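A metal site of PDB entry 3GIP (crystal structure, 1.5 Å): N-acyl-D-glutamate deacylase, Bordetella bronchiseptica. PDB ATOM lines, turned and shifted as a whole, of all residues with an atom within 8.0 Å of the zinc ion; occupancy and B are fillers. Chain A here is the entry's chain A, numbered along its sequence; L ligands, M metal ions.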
ATOM      1  N   HIS A  66     -12.358  25.257  19.233  1.00  0.00           N
ATOM      2  CA  HIS A  66     -12.845  24.282  20.195  1.00  0.00           C
ATOM      3  C   HIS A  66     -13.686  24.879  21.299  1.00  0.00           C
ATOM      4  O   HIS A  66     -13.241  25.002  22.449  1.00  0.00           O
ATOM      5  CB  HIS A  66     -11.698  23.483  20.815  1.00  0.00           C
ATOM      6  CG  HIS A  66     -12.143  22.184  21.405  1.00  0.00           C
ATOM      7  ND1 HIS A  66     -12.071  20.992  20.719  1.00  0.00           N
ATOM      8  CD2 HIS A  66     -12.759  21.900  22.573  1.00  0.00           C
ATOM      9  CE1 HIS A  66     -12.618  20.030  21.440  1.00  0.00           C
ATOM     10  NE2 HIS A  66     -13.046  20.558  22.575  1.00  0.00           N
ATOM     11  N   HIS A  68     -17.463  25.057  23.536  1.00  0.00           N
ATOM     12  CA  HIS A  68     -18.563  24.256  24.061  1.00  0.00           C
ATOM     13  C   HIS A  68     -19.660  25.238  24.432  1.00  0.00           C
ATOM     14  O   HIS A  68     -20.488  24.975  25.304  1.00  0.00           O
ATOM     15  CB  HIS A  68     -18.150  23.477  25.313  1.00  0.00           C
ATOM     16  CG  HIS A  68     -17.321  22.263  25.027  1.00  0.00           C
ATOM     17  ND1 HIS A  68     -17.786  21.209  24.265  1.00  0.00           N
ATOM     18  CD2 HIS A  68     -16.072  21.921  25.421  1.00  0.00           C
ATOM     19  CE1 HIS A  68     -16.852  20.276  24.198  1.00  0.00           C
ATOM     20  NE2 HIS A  68     -15.812  20.686  24.890  1.00  0.00           N
ATOM     21  N   ASN A  94     -18.403  20.399  20.012  1.00  0.00           N
ATOM     22  CA  ASN A  94     -17.236  19.535  20.086  1.00  0.00           C
ATOM     23  C   ASN A  94     -17.347  18.348  21.039  1.00  0.00           C
ATOM     24  O   ASN A  94     -18.234  18.293  21.893  1.00  0.00           O
ATOM     25  CB  ASN A  94     -16.017  20.373  20.456  1.00  0.00           C
ATOM     26  CG  ASN A  94     -15.516  21.203  19.304  1.00  0.00           C
ATOM     27  OD1 ASN A  94     -14.882  20.680  18.395  1.00  0.00           O
ATOM     28  ND2 ASN A  94     -15.803  22.497  19.335  1.00  0.00           N
ATOM     29  N   CYS A  95     -16.411  17.421  20.879  1.00  0.00           N
ATOM     30  CA  CYS A  95     -16.298  16.233  21.719  1.00  0.00           C
ATOM     31  C   CYS A  95     -17.529  15.346  21.770  1.00  0.00           C
ATOM     32  O   CYS A  95     -17.782  14.691  22.769  1.00  0.00           O
ATOM     33  CB  CYS A  95     -15.918  16.647  23.139  1.00  0.00           C
ATOM     34  SG  CYS A  95     -14.469  17.770  23.153  1.00  0.00           S
ATOM     35  N   GLY A  96     -18.285  15.341  20.672  1.00  0.00           N
ATOM     36  CA  GLY A  96     -19.472  14.504  20.604  1.00  0.00           C
ATOM     37  C   GLY A  96     -20.759  15.098  21.125  1.00  0.00           C
ATOM     38  O   GLY A  96     -21.818  14.504  20.943  1.00  0.00           O
ATOM     39  N   VAL A  97     -20.689  16.267  21.766  1.00  0.00           N
ATOM     40  CA  VAL A  97     -21.894  16.887  22.311  1.00  0.00           C
ATOM     41  C   VAL A  97     -22.204  18.233  21.670  1.00  0.00           C
ATOM     42  O   VAL A  97     -21.343  19.113  21.592  1.00  0.00           O
ATOM     43  CB  VAL A  97     -21.800  17.040  23.845  1.00  0.00           C
ATOM     44  CG1 VAL A  97     -21.838  15.670  24.499  1.00  0.00           C
ATOM     45  CG2 VAL A  97     -20.527  17.780  24.233  1.00  0.00           C
ATOM     46  N   LEU A 114     -21.210  19.339  29.681  1.00  0.00           N
ATOM     47  CA  LEU A 114     -20.222  20.262  29.128  1.00  0.00           C
ATOM     48  C   LEU A 114     -20.942  21.385  28.381  1.00  0.00           C
ATOM     49  O   LEU A 114     -20.317  22.382  28.016  1.00  0.00           O
ATOM     50  CB  LEU A 114     -19.288  19.524  28.156  1.00  0.00           C
ATOM     51  CG  LEU A 114     -18.421  18.390  28.714  1.00  0.00           C
ATOM     52  CD1 LEU A 114     -17.651  17.739  27.577  1.00  0.00           C
ATOM     53  CD2 LEU A 114     -17.474  18.934  29.776  1.00  0.00           C
ATOM     54  N   THR A 186     -16.674  13.633  17.621  1.00  0.00           N
ATOM     55  CA  THR A 186     -16.790  12.426  18.418  1.00  0.00           C
ATOM     56  C   THR A 186     -16.150  12.660  19.780  1.00  0.00           C
ATOM     57  O   THR A 186     -15.268  13.523  19.927  1.00  0.00           O
ATOM     58  CB  THR A 186     -16.091  11.207  17.753  1.00  0.00           C
ATOM     59  OG1 THR A 186     -14.770  11.571  17.329  1.00  0.00           O
ATOM     60  CG2 THR A 186     -16.898  10.725  16.562  1.00  0.00           C
ATOM     61  N   GLY A 187     -16.638  11.920  20.772  1.00  0.00           N
ATOM     62  CA  GLY A 187     -16.108  12.001  22.127  1.00  0.00           C
ATOM     63  C   GLY A 187     -15.923  10.541  22.505  1.00  0.00           C
ATOM     64  O   GLY A 187     -16.676   9.991  23.318  1.00  0.00           O
ATOM     65  N   LEU A 188     -14.921   9.913  21.912  1.00  0.00           N
ATOM     66  CA  LEU A 188     -14.668   8.491  22.117  1.00  0.00           C
ATOM     67  C   LEU A 188     -14.240   8.100  23.530  1.00  0.00           C
ATOM     68  O   LEU A 188     -14.254   6.915  23.873  1.00  0.00           O
ATOM     69  CB  LEU A 188     -13.654   7.992  21.081  1.00  0.00           C
ATOM     70  CG  LEU A 188     -14.064   8.302  19.628  1.00  0.00           C
ATOM     71  CD1 LEU A 188     -13.078   7.661  18.673  1.00  0.00           C
ATOM     72  CD2 LEU A 188     -15.482   7.788  19.353  1.00  0.00           C
ATOM     73  N   ALA A 189     -13.881   9.082  24.348  1.00  0.00           N
ATOM     74  CA  ALA A 189     -13.481   8.817  25.720  1.00  0.00           C
ATOM     75  C   ALA A 189     -14.704   8.876  26.628  1.00  0.00           C
ATOM     76  O   ALA A 189     -14.613   8.586  27.821  1.00  0.00           O
ATOM     77  CB  ALA A 189     -12.453   9.867  26.178  1.00  0.00           C
ATOM     78  N   TYR A 190     -15.851   9.246  26.057  1.00  0.00           N
ATOM     79  CA  TYR A 190     -17.098   9.375  26.810  1.00  0.00           C
ATOM     80  C   TYR A 190     -18.208   8.446  26.349  1.00  0.00           C
ATOM     81  O   TYR A 190     -18.201   7.928  25.229  1.00  0.00           O
ATOM     82  CB  TYR A 190     -17.651  10.791  26.688  1.00  0.00           C
ATOM     83  CG  TYR A 190     -16.713  11.896  27.097  1.00  0.00           C
ATOM     84  CD1 TYR A 190     -16.162  11.937  28.372  1.00  0.00           C
ATOM     85  CD2 TYR A 190     -16.421  12.940  26.209  1.00  0.00           C
ATOM     86  CE1 TYR A 190     -15.339  12.986  28.767  1.00  0.00           C
ATOM     87  CE2 TYR A 190     -15.603  13.986  26.591  1.00  0.00           C
ATOM     88  CZ  TYR A 190     -15.066  14.010  27.868  1.00  0.00           C
ATOM     89  OH  TYR A 190     -14.260  15.061  28.253  1.00  0.00           O
ATOM     90  N   SER A 217     -12.325  15.186  16.576  1.00  0.00           N
ATOM     91  CA  SER A 217     -12.410  14.152  17.594  1.00  0.00           C
ATOM     92  C   SER A 217     -11.682  14.303  18.911  1.00  0.00           C
ATOM     93  O   SER A 217     -10.502  14.672  18.959  1.00  0.00           O
ATOM     94  CB  SER A 217     -11.974  12.817  16.970  1.00  0.00           C
ATOM     95  OG  SER A 217     -12.021  11.752  17.924  1.00  0.00           O
ATOM     96  N   HIS A 218     -12.418  14.039  19.986  1.00  0.00           N
ATOM     97  CA  HIS A 218     -11.839  14.001  21.317  1.00  0.00           C
ATOM     98  C   HIS A 218     -11.622  12.485  21.267  1.00  0.00           C
ATOM     99  O   HIS A 218     -12.574  11.706  21.381  1.00  0.00           O
ATOM    100  CB  HIS A 218     -12.873  14.385  22.381  1.00  0.00           C
ATOM    101  CG  HIS A 218     -12.394  14.136  23.780  1.00  0.00           C
ATOM    102  ND1 HIS A 218     -12.601  15.033  24.810  1.00  0.00           N
ATOM    103  CD2 HIS A 218     -11.763  13.071  24.336  1.00  0.00           C
ATOM    104  CE1 HIS A 218     -12.101  14.535  25.926  1.00  0.00           C
ATOM    105  NE2 HIS A 218     -11.595  13.349  25.665  1.00  0.00           N
ATOM    106  N   ILE A 219     -10.384  12.077  21.044  1.00  0.00           N
ATOM    107  CA  ILE A 219     -10.055  10.671  20.892  1.00  0.00           C
ATOM    108  C   ILE A 219     -10.357   9.745  22.064  1.00  0.00           C
ATOM    109  O   ILE A 219     -10.615  10.187  23.190  1.00  0.00           O
ATOM    110  CB  ILE A 219      -8.592  10.521  20.403  1.00  0.00           C
ATOM    111  CG1 ILE A 219      -7.609  11.028  21.449  1.00  0.00           C
ATOM    112  CG2 ILE A 219      -8.420  11.322  19.111  1.00  0.00           C
ATOM    113  CD1 ILE A 219      -6.166  10.966  20.984  1.00  0.00           C
ATOM    114  N   GLU A 222      -6.421   9.610  26.061  1.00  0.00           N
ATOM    115  CA  GLU A 222      -5.337  10.568  25.918  1.00  0.00           C
ATOM    116  C   GLU A 222      -4.222  10.338  26.941  1.00  0.00           C
ATOM    117  O   GLU A 222      -3.463  11.244  27.263  1.00  0.00           O
ATOM    118  CB  GLU A 222      -5.891  11.985  26.028  1.00  0.00           C
ATOM    119  CG  GLU A 222      -6.953  12.273  24.958  1.00  0.00           C
ATOM    120  CD  GLU A 222      -7.409  13.717  24.923  1.00  0.00           C
ATOM    121  OE1 GLU A 222      -8.107  14.150  25.866  1.00  0.00           O
ATOM    122  OE2 GLU A 222      -7.063  14.419  23.956  1.00  0.00           O
ATOM    123  N   SER A 247      -8.836  16.987  18.377  1.00  0.00           N
ATOM    124  CA  SER A 247      -9.126  17.982  19.400  1.00  0.00           C
ATOM    125  C   SER A 247      -8.187  17.962  20.599  1.00  0.00           C
ATOM    126  O   SER A 247      -7.712  16.904  21.016  1.00  0.00           O
ATOM    127  CB  SER A 247     -10.558  17.814  19.906  1.00  0.00           C
ATOM    128  OG  SER A 247     -11.488  17.993  18.855  1.00  0.00           O
ATOM    129  N   HIS A 248      -7.941  19.158  21.140  1.00  0.00           N
ATOM    130  CA  HIS A 248      -7.095  19.344  22.318  1.00  0.00           C
ATOM    131  C   HIS A 248      -6.076  18.231  22.502  1.00  0.00           C
ATOM    132  O   HIS A 248      -6.093  17.506  23.503  1.00  0.00           O
ATOM    133  CB  HIS A 248      -7.958  19.507  23.581  1.00  0.00           C
ATOM    134  CG  HIS A 248      -9.085  18.513  23.709  1.00  0.00           C
ATOM    135  ND1 HIS A 248      -8.901  17.152  23.639  1.00  0.00           N
ATOM    136  CD2 HIS A 248     -10.402  18.698  23.979  1.00  0.00           C
ATOM    137  CE1 HIS A 248     -10.039  16.536  23.862  1.00  0.00           C
ATOM    138  NE2 HIS A 248     -10.968  17.455  24.076  1.00  0.00           N
ATOM    139  N   LYS A 250      -3.059  16.093  23.470  1.00  0.00           N
ATOM    140  CA  LYS A 250      -2.246  16.104  24.684  1.00  0.00           C
ATOM    141  C   LYS A 250      -1.859  14.684  25.074  1.00  0.00           C
ATOM    142  O   LYS A 250      -2.403  13.710  24.546  1.00  0.00           O
ATOM    143  CB  LYS A 250      -3.065  16.684  25.828  1.00  0.00           C
ATOM    144  CG  LYS A 250      -4.222  15.750  26.244  1.00  0.00           C
ATOM    145  CD  LYS A 250      -5.052  16.323  27.386  1.00  0.00           C
ATOM    146  CE  LYS A 250      -6.059  17.332  26.890  1.00  0.00           C
ATOM    147  NZ  LYS A 250      -7.154  16.699  26.081  1.00  0.00           N
ATOM    148  N   TYR A 282      -4.933  24.032  23.886  1.00  0.00           N
ATOM    149  CA  TYR A 282      -5.137  25.208  24.721  1.00  0.00           C
ATOM    150  C   TYR A 282      -3.784  25.240  25.434  1.00  0.00           C
ATOM    151  O   TYR A 282      -3.199  24.191  25.698  1.00  0.00           O
ATOM    152  CB  TYR A 282      -6.331  25.047  25.685  1.00  0.00           C
ATOM    153  CG  TYR A 282      -6.469  23.717  26.373  1.00  0.00           C
ATOM    154  CD1 TYR A 282      -5.660  23.379  27.461  1.00  0.00           C
ATOM    155  CD2 TYR A 282      -7.411  22.789  25.936  1.00  0.00           C
ATOM    156  CE1 TYR A 282      -5.803  22.156  28.102  1.00  0.00           C
ATOM    157  CE2 TYR A 282      -7.563  21.567  26.573  1.00  0.00           C
ATOM    158  CZ  TYR A 282      -6.757  21.249  27.651  1.00  0.00           C
ATOM    159  OH  TYR A 282      -6.900  20.042  28.274  1.00  0.00           O
ATOM    160  N   SER A 288      -9.703  19.637  31.782  1.00  0.00           N
ATOM    161  CA  SER A 288     -10.878  19.873  32.603  1.00  0.00           C
ATOM    162  C   SER A 288     -12.097  19.264  31.939  1.00  0.00           C
ATOM    163  O   SER A 288     -12.376  19.533  30.780  1.00  0.00           O
ATOM    164  CB  SER A 288     -11.111  21.366  32.817  1.00  0.00           C
ATOM    165  OG  SER A 288     -12.202  21.589  33.715  1.00  0.00           O
ATOM    166  N   THR A 289     -12.803  18.431  32.680  1.00  0.00           N
ATOM    167  CA  THR A 289     -14.010  17.802  32.147  1.00  0.00           C
ATOM    168  C   THR A 289     -14.779  17.220  33.326  1.00  0.00           C
ATOM    169  O   THR A 289     -14.564  17.623  34.461  1.00  0.00           O
ATOM    170  CB  THR A 289     -13.663  16.699  31.110  1.00  0.00           C
ATOM    171  OG1 THR A 289     -14.870  16.196  30.525  1.00  0.00           O
ATOM    172  CG2 THR A 289     -12.903  15.550  31.768  1.00  0.00           C
ATOM    173  N   ASP A 365     -11.551  25.445  24.602  1.00  0.00           N
ATOM    174  CA  ASP A 365     -12.217  24.379  25.327  1.00  0.00           C
ATOM    175  C   ASP A 365     -12.780  24.912  26.646  1.00  0.00           C
ATOM    176  O   ASP A 365     -12.803  24.217  27.667  1.00  0.00           O
ATOM    177  CB  ASP A 365     -11.262  23.206  25.578  1.00  0.00           C
ATOM    178  CG  ASP A 365     -11.989  21.912  25.895  1.00  0.00           C
ATOM    179  OD1 ASP A 365     -13.233  21.880  25.786  1.00  0.00           O
ATOM    180  OD2 ASP A 365     -11.323  20.916  26.241  1.00  0.00           O
ATOM    181  N   LEU A 367     -15.337  25.965  29.494  1.00  0.00           N
ATOM    182  CA  LEU A 367     -16.573  25.369  29.993  1.00  0.00           C
ATOM    183  C   LEU A 367     -17.258  26.478  30.779  1.00  0.00           C
ATOM    184  O   LEU A 367     -17.117  26.580  31.994  1.00  0.00           O
ATOM    185  CB  LEU A 367     -16.253  24.157  30.885  1.00  0.00           C
ATOM    186  CG  LEU A 367     -15.550  23.013  30.144  1.00  0.00           C
ATOM    187  CD1 LEU A 367     -15.138  21.927  31.117  1.00  0.00           C
ATOM    188  CD2 LEU A 367     -16.484  22.451  29.072  1.00  0.00           C
ATOM    189  N   ARG A 376      -8.649  28.542  30.999  1.00  0.00           N
ATOM    190  CA  ARG A 376      -8.578  28.536  29.544  1.00  0.00           C
ATOM    191  C   ARG A 376      -9.836  29.197  28.969  1.00  0.00           C
ATOM    192  O   ARG A 376      -9.825  29.692  27.839  1.00  0.00           O
ATOM    193  CB  ARG A 376      -8.449  27.096  29.030  1.00  0.00           C
ATOM    194  CG  ARG A 376      -9.668  26.235  29.297  1.00  0.00           C
ATOM    195  CD  ARG A 376      -9.344  24.767  29.110  1.00  0.00           C
ATOM    196  NE  ARG A 376     -10.546  23.945  29.193  1.00  0.00           N
ATOM    197  CZ  ARG A 376     -10.539  22.619  29.289  1.00  0.00           C
ATOM    198  NH1 ARG A 376      -9.397  21.955  29.317  1.00  0.00           N
ATOM    199  NH2 ARG A 376     -11.690  21.957  29.340  1.00  0.00           N
HETATM  200  C1  LIG L   1     -13.647  18.204  26.870  1.00  0.00           C
HETATM  201  O1  LIG L   1     -13.908  17.044  26.668  1.00  0.00           O
HETATM  202  O2  LIG L   1     -12.891  18.876  25.996  1.00  0.00           O
HETATM  203  C2  LIG L   1     -14.155  18.891  28.102  1.00  0.00           C
HETATM  204 ZN    ZN M   1     -12.967  17.005  24.596  1.00  0.00          ZN
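A ring nitrogen (ND1) of His 248 lies within hydrogen-bond range of the side-chain carboxylate of Glu 222 (3.3 Å).
The side-chain amino group (NZ) of Lys 250 is in hydrogen-bond range of the backbone carbonyl oxygen (O) of His 248 (2.9 Å).
NE2 of His 68 sits close to SG of Cys 95, 3.7 Å away.
SG of Cys 95 sits close to NE2 of His 66 (3.2 Å).
N of His 218 is in hydrogen-bond range of O of Thr 186, 2.9 Å away.
The backbone carbonyl oxygen of His 218 is in hydrogen-bond range of the backbone NH of Leu 188, at 3.0 Å.
Three residues have an atom within 4 Å of the zinc ion: Cys 95, His 218 and His 248.
The nearest printed residue that does not touch the zinc ion is His 66 (4.1 Å).
The zinc ion is bound by a ring nitrogen (ND1) of His 218 (2.0 Å).
The zinc ion is bound by NE2 of His 248, at 2.1 Å.
The side-chain sulfur (SG) of Cys 95 is bound to the zinc ion (2.2 Å).
O1 of the ligand binds the zinc ion.
The zinc ion is bound by an oxygen (O2) of the ligand, 2.3 Å away.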
